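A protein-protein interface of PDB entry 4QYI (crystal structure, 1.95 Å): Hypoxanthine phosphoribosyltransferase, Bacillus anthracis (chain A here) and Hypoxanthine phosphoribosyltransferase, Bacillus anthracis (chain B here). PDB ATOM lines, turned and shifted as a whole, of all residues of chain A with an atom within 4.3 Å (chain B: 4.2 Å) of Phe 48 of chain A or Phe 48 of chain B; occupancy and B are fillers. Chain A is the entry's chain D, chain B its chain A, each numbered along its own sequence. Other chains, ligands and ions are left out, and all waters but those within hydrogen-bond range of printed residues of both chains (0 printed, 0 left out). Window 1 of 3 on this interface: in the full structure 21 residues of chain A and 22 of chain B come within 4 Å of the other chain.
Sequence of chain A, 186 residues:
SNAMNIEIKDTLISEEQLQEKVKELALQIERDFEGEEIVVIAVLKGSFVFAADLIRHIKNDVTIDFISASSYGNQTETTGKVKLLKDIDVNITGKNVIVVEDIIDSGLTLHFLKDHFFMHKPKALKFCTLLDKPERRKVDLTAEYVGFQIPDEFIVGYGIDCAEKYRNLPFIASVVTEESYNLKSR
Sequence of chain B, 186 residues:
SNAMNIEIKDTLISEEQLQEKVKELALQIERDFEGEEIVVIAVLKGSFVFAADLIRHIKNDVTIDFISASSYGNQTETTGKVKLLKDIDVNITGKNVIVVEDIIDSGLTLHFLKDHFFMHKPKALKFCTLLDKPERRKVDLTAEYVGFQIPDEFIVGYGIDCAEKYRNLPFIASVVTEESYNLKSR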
ATOM      1  N   LYS A  45      -0.906  21.056  18.944  1.00  0.00           N
ATOM      2  CA  LYS A  45      -0.387  20.719  17.621  1.00  0.00           C
ATOM      3  C   LYS A  45       0.527  21.806  17.073  1.00  0.00           C
ATOM      4  O   LYS A  45       1.439  21.534  16.295  1.00  0.00           O
ATOM      5  CB  LYS A  45      -1.548  20.586  16.634  1.00  0.00           C
ATOM      6  CG  LYS A  45      -2.503  19.455  16.943  1.00  0.00           C
ATOM      7  CD  LYS A  45      -3.766  19.449  16.107  1.00  0.00           C
ATOM      8  CE  LYS A  45      -4.671  18.326  16.599  1.00  0.00           C
ATOM      9  NZ  LYS A  45      -5.936  18.244  15.829  1.00  0.00           N
ATOM     10  N   GLY A  46       0.280  23.029  17.515  1.00  0.00           N
ATOM     11  CA  GLY A  46       0.932  24.213  16.954  1.00  0.00           C
ATOM     12  C   GLY A  46       2.427  24.412  16.948  1.00  0.00           C
ATOM     13  O   GLY A  46       2.938  25.200  16.175  1.00  0.00           O
ATOM     14  N   SER A  47       3.138  23.702  17.795  1.00  0.00           N
ATOM     15  CA  SER A  47       4.537  23.845  17.836  1.00  0.00           C
ATOM     16  C   SER A  47       5.273  22.884  16.912  1.00  0.00           C
ATOM     17  O   SER A  47       6.500  22.958  16.842  1.00  0.00           O
ATOM     18  CB  SER A  47       4.978  23.554  19.268  1.00  0.00           C
ATOM     19  OG  SER A  47       4.821  22.182  19.528  1.00  0.00           O
ATOM     20  N   PHE A  48       4.570  22.017  16.173  1.00  0.00           N
ATOM     21  CA  PHE A  48       5.286  20.969  15.407  1.00  0.00           C
ATOM     22  C   PHE A  48       6.214  21.472  14.309  1.00  0.00           C
ATOM     23  O   PHE A  48       7.238  20.856  14.074  1.00  0.00           O
ATOM     24  CB  PHE A  48       4.363  19.863  14.894  1.00  0.00           C
ATOM     25  CG  PHE A  48       3.773  20.098  13.542  1.00  0.00           C
ATOM     26  CD1 PHE A  48       2.670  20.920  13.374  1.00  0.00           C
ATOM     27  CD2 PHE A  48       4.287  19.443  12.436  1.00  0.00           C
ATOM     28  CE1 PHE A  48       2.111  21.117  12.117  1.00  0.00           C
ATOM     29  CE2 PHE A  48       3.731  19.640  11.174  1.00  0.00           C
ATOM     30  CZ  PHE A  48       2.647  20.476  11.014  1.00  0.00           C
ATOM     31  N   VAL A  49       5.877  22.582  13.673  1.00  0.00           N
ATOM     32  CA  VAL A  49       6.726  23.124  12.610  1.00  0.00           C
ATOM     33  C   VAL A  49       7.985  23.727  13.226  1.00  0.00           C
ATOM     34  O   VAL A  49       9.099  23.460  12.797  1.00  0.00           O
ATOM     35  CB  VAL A  49       5.985  24.154  11.768  1.00  0.00           C
ATOM     36  CG1 VAL A  49       6.917  24.762  10.741  1.00  0.00           C
ATOM     37  CG2 VAL A  49       4.786  23.499  11.080  1.00  0.00           C
ATOM     38  N   PHE A  50       7.792  24.552  14.237  1.00  0.00           N
ATOM     39  CA  PHE A  50       8.896  25.160  14.968  1.00  0.00           C
ATOM     40  C   PHE A  50       9.847  24.085  15.511  1.00  0.00           C
ATOM     41  O   PHE A  50      11.079  24.197  15.389  1.00  0.00           O
ATOM     42  CB  PHE A  50       8.295  26.003  16.101  1.00  0.00           C
ATOM     43  CG  PHE A  50       9.306  26.626  17.040  1.00  0.00           C
ATOM     44  CD1 PHE A  50      10.460  27.213  16.570  1.00  0.00           C
ATOM     45  CD2 PHE A  50       9.001  26.738  18.381  1.00  0.00           C
ATOM     46  CE1 PHE A  50      11.359  27.809  17.443  1.00  0.00           C
ATOM     47  CE2 PHE A  50       9.874  27.330  19.259  1.00  0.00           C
ATOM     48  CZ  PHE A  50      11.060  27.880  18.788  1.00  0.00           C
ATOM     49  N   ALA A  51       9.270  23.026  16.076  1.00  0.00           N
ATOM     50  CA  ALA A  51      10.070  21.947  16.654  1.00  0.00           C
ATOM     51  C   ALA A  51      10.872  21.246  15.587  1.00  0.00           C
ATOM     52  O   ALA A  51      12.060  20.993  15.786  1.00  0.00           O
ATOM     53  CB  ALA A  51       9.203  20.948  17.391  1.00  0.00           C
ATOM     54  N   ALA A  52      10.243  20.945  14.461  1.00  0.00           N
ATOM     55  CA  ALA A  52      10.935  20.289  13.357  1.00  0.00           C
ATOM     56  C   ALA A  52      12.150  21.123  12.910  1.00  0.00           C
ATOM     57  O   ALA A  52      13.218  20.572  12.698  1.00  0.00           O
ATOM     58  CB  ALA A  52       9.987  20.060  12.180  1.00  0.00           C
ATOM     59  N   ILE A  55      15.041  21.526  16.096  1.00  0.00           N
ATOM     60  CA  ILE A  55      15.878  20.371  16.408  1.00  0.00           C
ATOM     61  C   ILE A  55      16.923  20.051  15.351  1.00  0.00           C
ATOM     62  O   ILE A  55      17.989  19.517  15.676  1.00  0.00           O
ATOM     63  CB  ILE A  55      15.067  19.126  16.783  1.00  0.00           C
ATOM     64  CG1 ILE A  55      14.321  18.549  15.576  1.00  0.00           C
ATOM     65  CG2 ILE A  55      14.134  19.463  17.940  1.00  0.00           C
ATOM     66  CD1 ILE A  55      13.585  17.268  15.895  1.00  0.00           C
ATOM     67  N   ILE A  64      12.955  13.460  20.986  1.00  0.00           N
ATOM     68  CA  ILE A  64      11.782  14.325  20.937  1.00  0.00           C
ATOM     69  C   ILE A  64      10.517  13.543  21.205  1.00  0.00           C
ATOM     70  O   ILE A  64      10.428  12.358  20.878  1.00  0.00           O
ATOM     71  CB  ILE A  64      11.694  15.162  19.645  1.00  0.00           C
ATOM     72  CG1 ILE A  64      10.478  16.111  19.730  1.00  0.00           C
ATOM     73  CG2 ILE A  64      11.574  14.279  18.422  1.00  0.00           C
ATOM     74  CD1 ILE A  64      10.503  17.250  18.742  1.00  0.00           C
ATOM     75  N   PHE A  66       6.015  14.236  22.241  1.00  0.00           N
ATOM     76  CA  PHE A  66       4.922  15.169  22.179  1.00  0.00           C
ATOM     77  C   PHE A  66       3.959  15.023  23.331  1.00  0.00           C
ATOM     78  O   PHE A  66       3.835  13.961  23.926  1.00  0.00           O
ATOM     79  CB  PHE A  66       4.165  14.946  20.880  1.00  0.00           C
ATOM     80  CG  PHE A  66       5.011  15.104  19.664  1.00  0.00           C
ATOM     81  CD1 PHE A  66       5.287  16.368  19.176  1.00  0.00           C
ATOM     82  CD2 PHE A  66       5.527  14.006  19.008  1.00  0.00           C
ATOM     83  CE1 PHE A  66       6.063  16.533  18.054  1.00  0.00           C
ATOM     84  CE2 PHE A  66       6.307  14.160  17.883  1.00  0.00           C
ATOM     85  CZ  PHE A  66       6.573  15.428  17.404  1.00  0.00           C
ATOM     86  N   LYS B  45       5.174   8.988  15.082  1.00  0.00           N
ATOM     87  CA  LYS B  45       5.863  10.265  15.264  1.00  0.00           C
ATOM     88  C   LYS B  45       6.764  10.611  14.097  1.00  0.00           C
ATOM     89  O   LYS B  45       6.982  11.783  13.808  1.00  0.00           O
ATOM     90  CB  LYS B  45       6.775  10.175  16.486  1.00  0.00           C
ATOM     91  CG  LYS B  45       6.040   9.956  17.793  1.00  0.00           C
ATOM     92  CD  LYS B  45       6.966   9.658  18.975  1.00  0.00           C
ATOM     93  CE  LYS B  45       6.116   9.349  20.199  1.00  0.00           C
ATOM     94  NZ  LYS B  45       6.932   9.065  21.401  1.00  0.00           N
ATOM     95  N   GLY B  46       7.228   9.581  13.398  1.00  0.00           N
ATOM     96  CA  GLY B  46       8.218   9.717  12.348  1.00  0.00           C
ATOM     97  C   GLY B  46       7.997  10.570  11.123  1.00  0.00           C
ATOM     98  O   GLY B  46       8.951  10.955  10.460  1.00  0.00           O
ATOM     99  N   SER B  47       6.756  10.870  10.805  1.00  0.00           N
ATOM    100  CA  SER B  47       6.490  11.647   9.647  1.00  0.00           C
ATOM    101  C   SER B  47       6.404  13.141   9.942  1.00  0.00           C
ATOM    102  O   SER B  47       6.250  13.921   8.998  1.00  0.00           O
ATOM    103  CB  SER B  47       5.142  11.209   9.087  1.00  0.00           C
ATOM    104  OG  SER B  47       4.125  11.668   9.946  1.00  0.00           O
ATOM    105  N   PHE B  48       6.572  13.564  11.196  1.00  0.00           N
ATOM    106  CA  PHE B  48       6.367  14.990  11.528  1.00  0.00           C
ATOM    107  C   PHE B  48       7.298  15.972  10.844  1.00  0.00           C
ATOM    108  O   PHE B  48       6.860  17.067  10.522  1.00  0.00           O
ATOM    109  CB  PHE B  48       6.293  15.272  13.044  1.00  0.00           C
ATOM    110  CG  PHE B  48       7.605  15.579  13.718  1.00  0.00           C
ATOM    111  CD1 PHE B  48       8.491  14.575  14.084  1.00  0.00           C
ATOM    112  CD2 PHE B  48       7.929  16.895  14.039  1.00  0.00           C
ATOM    113  CE1 PHE B  48       9.684  14.876  14.714  1.00  0.00           C
ATOM    114  CE2 PHE B  48       9.115  17.199  14.680  1.00  0.00           C
ATOM    115  CZ  PHE B  48       9.986  16.183  15.028  1.00  0.00           C
ATOM    116  N   VAL B  49       8.541  15.585  10.583  1.00  0.00           N
ATOM    117  CA  VAL B  49       9.487  16.495   9.926  1.00  0.00           C
ATOM    118  C   VAL B  49       9.117  16.617   8.458  1.00  0.00           C
ATOM    119  O   VAL B  49       9.011  17.703   7.920  1.00  0.00           O
ATOM    120  CB  VAL B  49      10.946  16.029  10.100  1.00  0.00           C
ATOM    121  CG1 VAL B  49      11.877  16.927   9.319  1.00  0.00           C
ATOM    122  CG2 VAL B  49      11.330  16.012  11.574  1.00  0.00           C
ATOM    123  N   PHE B  50       8.909  15.479   7.818  1.00  0.00           N
ATOM    124  CA  PHE B  50       8.478  15.444   6.425  1.00  0.00           C
ATOM    125  C   PHE B  50       7.197  16.252   6.226  1.00  0.00           C
ATOM    126  O   PHE B  50       7.072  17.036   5.271  1.00  0.00           O
ATOM    127  CB  PHE B  50       8.302  13.989   6.041  1.00  0.00           C
ATOM    128  CG  PHE B  50       7.750  13.751   4.666  1.00  0.00           C
ATOM    129  CD1 PHE B  50       8.212  14.455   3.576  1.00  0.00           C
ATOM    130  CD2 PHE B  50       6.860  12.689   4.452  1.00  0.00           C
ATOM    131  CE1 PHE B  50       7.732  14.188   2.313  1.00  0.00           C
ATOM    132  CE2 PHE B  50       6.378  12.418   3.185  1.00  0.00           C
ATOM    133  CZ  PHE B  50       6.815  13.178   2.114  1.00  0.00           C
ATOM    134  N   ALA B  51       6.257  16.092   7.140  1.00  0.00           N
ATOM    135  CA  ALA B  51       4.968  16.784   7.031  1.00  0.00           C
ATOM    136  C   ALA B  51       5.149  18.271   7.152  1.00  0.00           C
ATOM    137  O   ALA B  51       4.559  19.018   6.377  1.00  0.00           O
ATOM    138  CB  ALA B  51       3.978  16.293   8.075  1.00  0.00           C
ATOM    139  N   ALA B  52       5.953  18.694   8.125  1.00  0.00           N
ATOM    140  CA  ALA B  52       6.207  20.111   8.322  1.00  0.00           C
ATOM    141  C   ALA B  52       6.783  20.721   7.031  1.00  0.00           C
ATOM    142  O   ALA B  52       6.358  21.784   6.613  1.00  0.00           O
ATOM    143  CB  ALA B  52       7.169  20.332   9.487  1.00  0.00           C
ATOM    144  N   ILE B  55       4.000  20.402   3.748  1.00  0.00           N
ATOM    145  CA  ILE B  55       2.867  21.330   3.719  1.00  0.00           C
ATOM    146  C   ILE B  55       3.230  22.776   3.424  1.00  0.00           C
ATOM    147  O   ILE B  55       2.412  23.523   2.862  1.00  0.00           O
ATOM    148  CB  ILE B  55       1.982  21.237   4.976  1.00  0.00           C
ATOM    149  CG1 ILE B  55       2.701  21.785   6.213  1.00  0.00           C
ATOM    150  CG2 ILE B  55       1.507  19.793   5.156  1.00  0.00           C
ATOM    151  CD1 ILE B  55       1.825  21.767   7.450  1.00  0.00           C
ATOM    152  N   ILE B  64      -4.256  20.274   8.804  1.00  0.00           N
ATOM    153  CA  ILE B  64      -3.428  19.125   9.164  1.00  0.00           C
ATOM    154  C   ILE B  64      -3.877  18.534  10.494  1.00  0.00           C
ATOM    155  O   ILE B  64      -4.321  19.241  11.371  1.00  0.00           O
ATOM    156  CB  ILE B  64      -1.903  19.404   9.105  1.00  0.00           C
ATOM    157  CG1 ILE B  64      -1.111  18.114   9.399  1.00  0.00           C
ATOM    158  CG2 ILE B  64      -1.506  20.481  10.080  1.00  0.00           C
ATOM    159  CD1 ILE B  64       0.342  18.160   8.968  1.00  0.00           C
ATOM    160  N   PHE B  66      -3.138  14.711  13.119  1.00  0.00           N
ATOM    161  CA  PHE B  66      -2.251  13.603  13.375  1.00  0.00           C
ATOM    162  C   PHE B  66      -2.976  12.354  13.859  1.00  0.00           C
ATOM    163  O   PHE B  66      -4.040  12.423  14.475  1.00  0.00           O
ATOM    164  CB  PHE B  66      -1.248  14.007  14.450  1.00  0.00           C
ATOM    165  CG  PHE B  66      -0.420  15.189  14.089  1.00  0.00           C
ATOM    166  CD1 PHE B  66       0.683  15.033  13.266  1.00  0.00           C
ATOM    167  CD2 PHE B  66      -0.732  16.445  14.561  1.00  0.00           C
ATOM    168  CE1 PHE B  66       1.456  16.111  12.907  1.00  0.00           C
ATOM    169  CE2 PHE B  66       0.044  17.542  14.206  1.00  0.00           C
ATOM    170  CZ  PHE B  66       1.135  17.372  13.376  1.00  0.00           C
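Phe 48 of chain B touches Phe 48 of chain A (O to CD2, 3.99 Å). CA of Ala 52 of chain B touches CE2 of Phe 48 of chain A (3.8 Å). Ile 55 of chain B touches Phe 48 of chain A. Ile 64 of chain B touches Phe 48 of chain A. CG of Phe 48 of chain A touches CZ of Phe 66 of chain B, at 3.8 Å. Ala 52 of chain A touches Phe 48 of chain B (CA to CE2, 3.8 Å). Ala 52 of chain B touches Ala 52 of chain A (CB to CB, 3.9 Å). CZ of Phe 48 of chain B touches CD1 of Ile 55 of chain A, 3.9 Å away. Phe 48 of chain B touches Ile 64 of chain A (CZ to CD1, 3.9 Å). CZ of Phe 66 of chain A touches CG of Phe 48 of chain B, 3.8 Å away.
Val 49 of chain A touches none of the printed residues of chain B. Of the printed residues of chain B, Ala 52 of chain A touches Phe 48 and Ala 52. Of the printed residues of chain B, Ile 55 of chain A touches Phe 48. Printed residues of chain A within 4 Å of Phe 48 of chain B: Phe 48 (3.99 Å), Ala 52 (3.8 Å), Ile 55 (3.9 Å), Ile 64 (3.9 Å) and Phe 66 (3.8 Å). Val 49 of chain B touches none of the printed residues of chain A. Of the printed residues of chain A, Ile 55 of chain B touches Phe 48. Printed residues of chain A within 4 Å of Ile 64 of chain B: Phe 48. Of the printed residues of chain A, Phe 66 of chain B touches Phe 48. The nearest printed residue of chain B that does not touch Phe 66 of chain A is Lys 45 of chain B (4.2 Å).
Printed residues of chain B that touch a printed residue of chain A: Phe 48, Ala 52, Ile 55, Ile 64 and Phe 66. Hydrophobic or aromatic side chains of chain B that line the printed part of chain A: Phe 48, Ala 52, Ile 55, Ile 64 and Phe 66. Of the 11 printed residues of chain A, 5 touch a printed residue of chain B. Hydrophobic or aromatic side chains of chain A within 4 Å of the printed part of chain B: Phe 48, Ala 52, Ile 55, Ile 64 and Phe 66.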
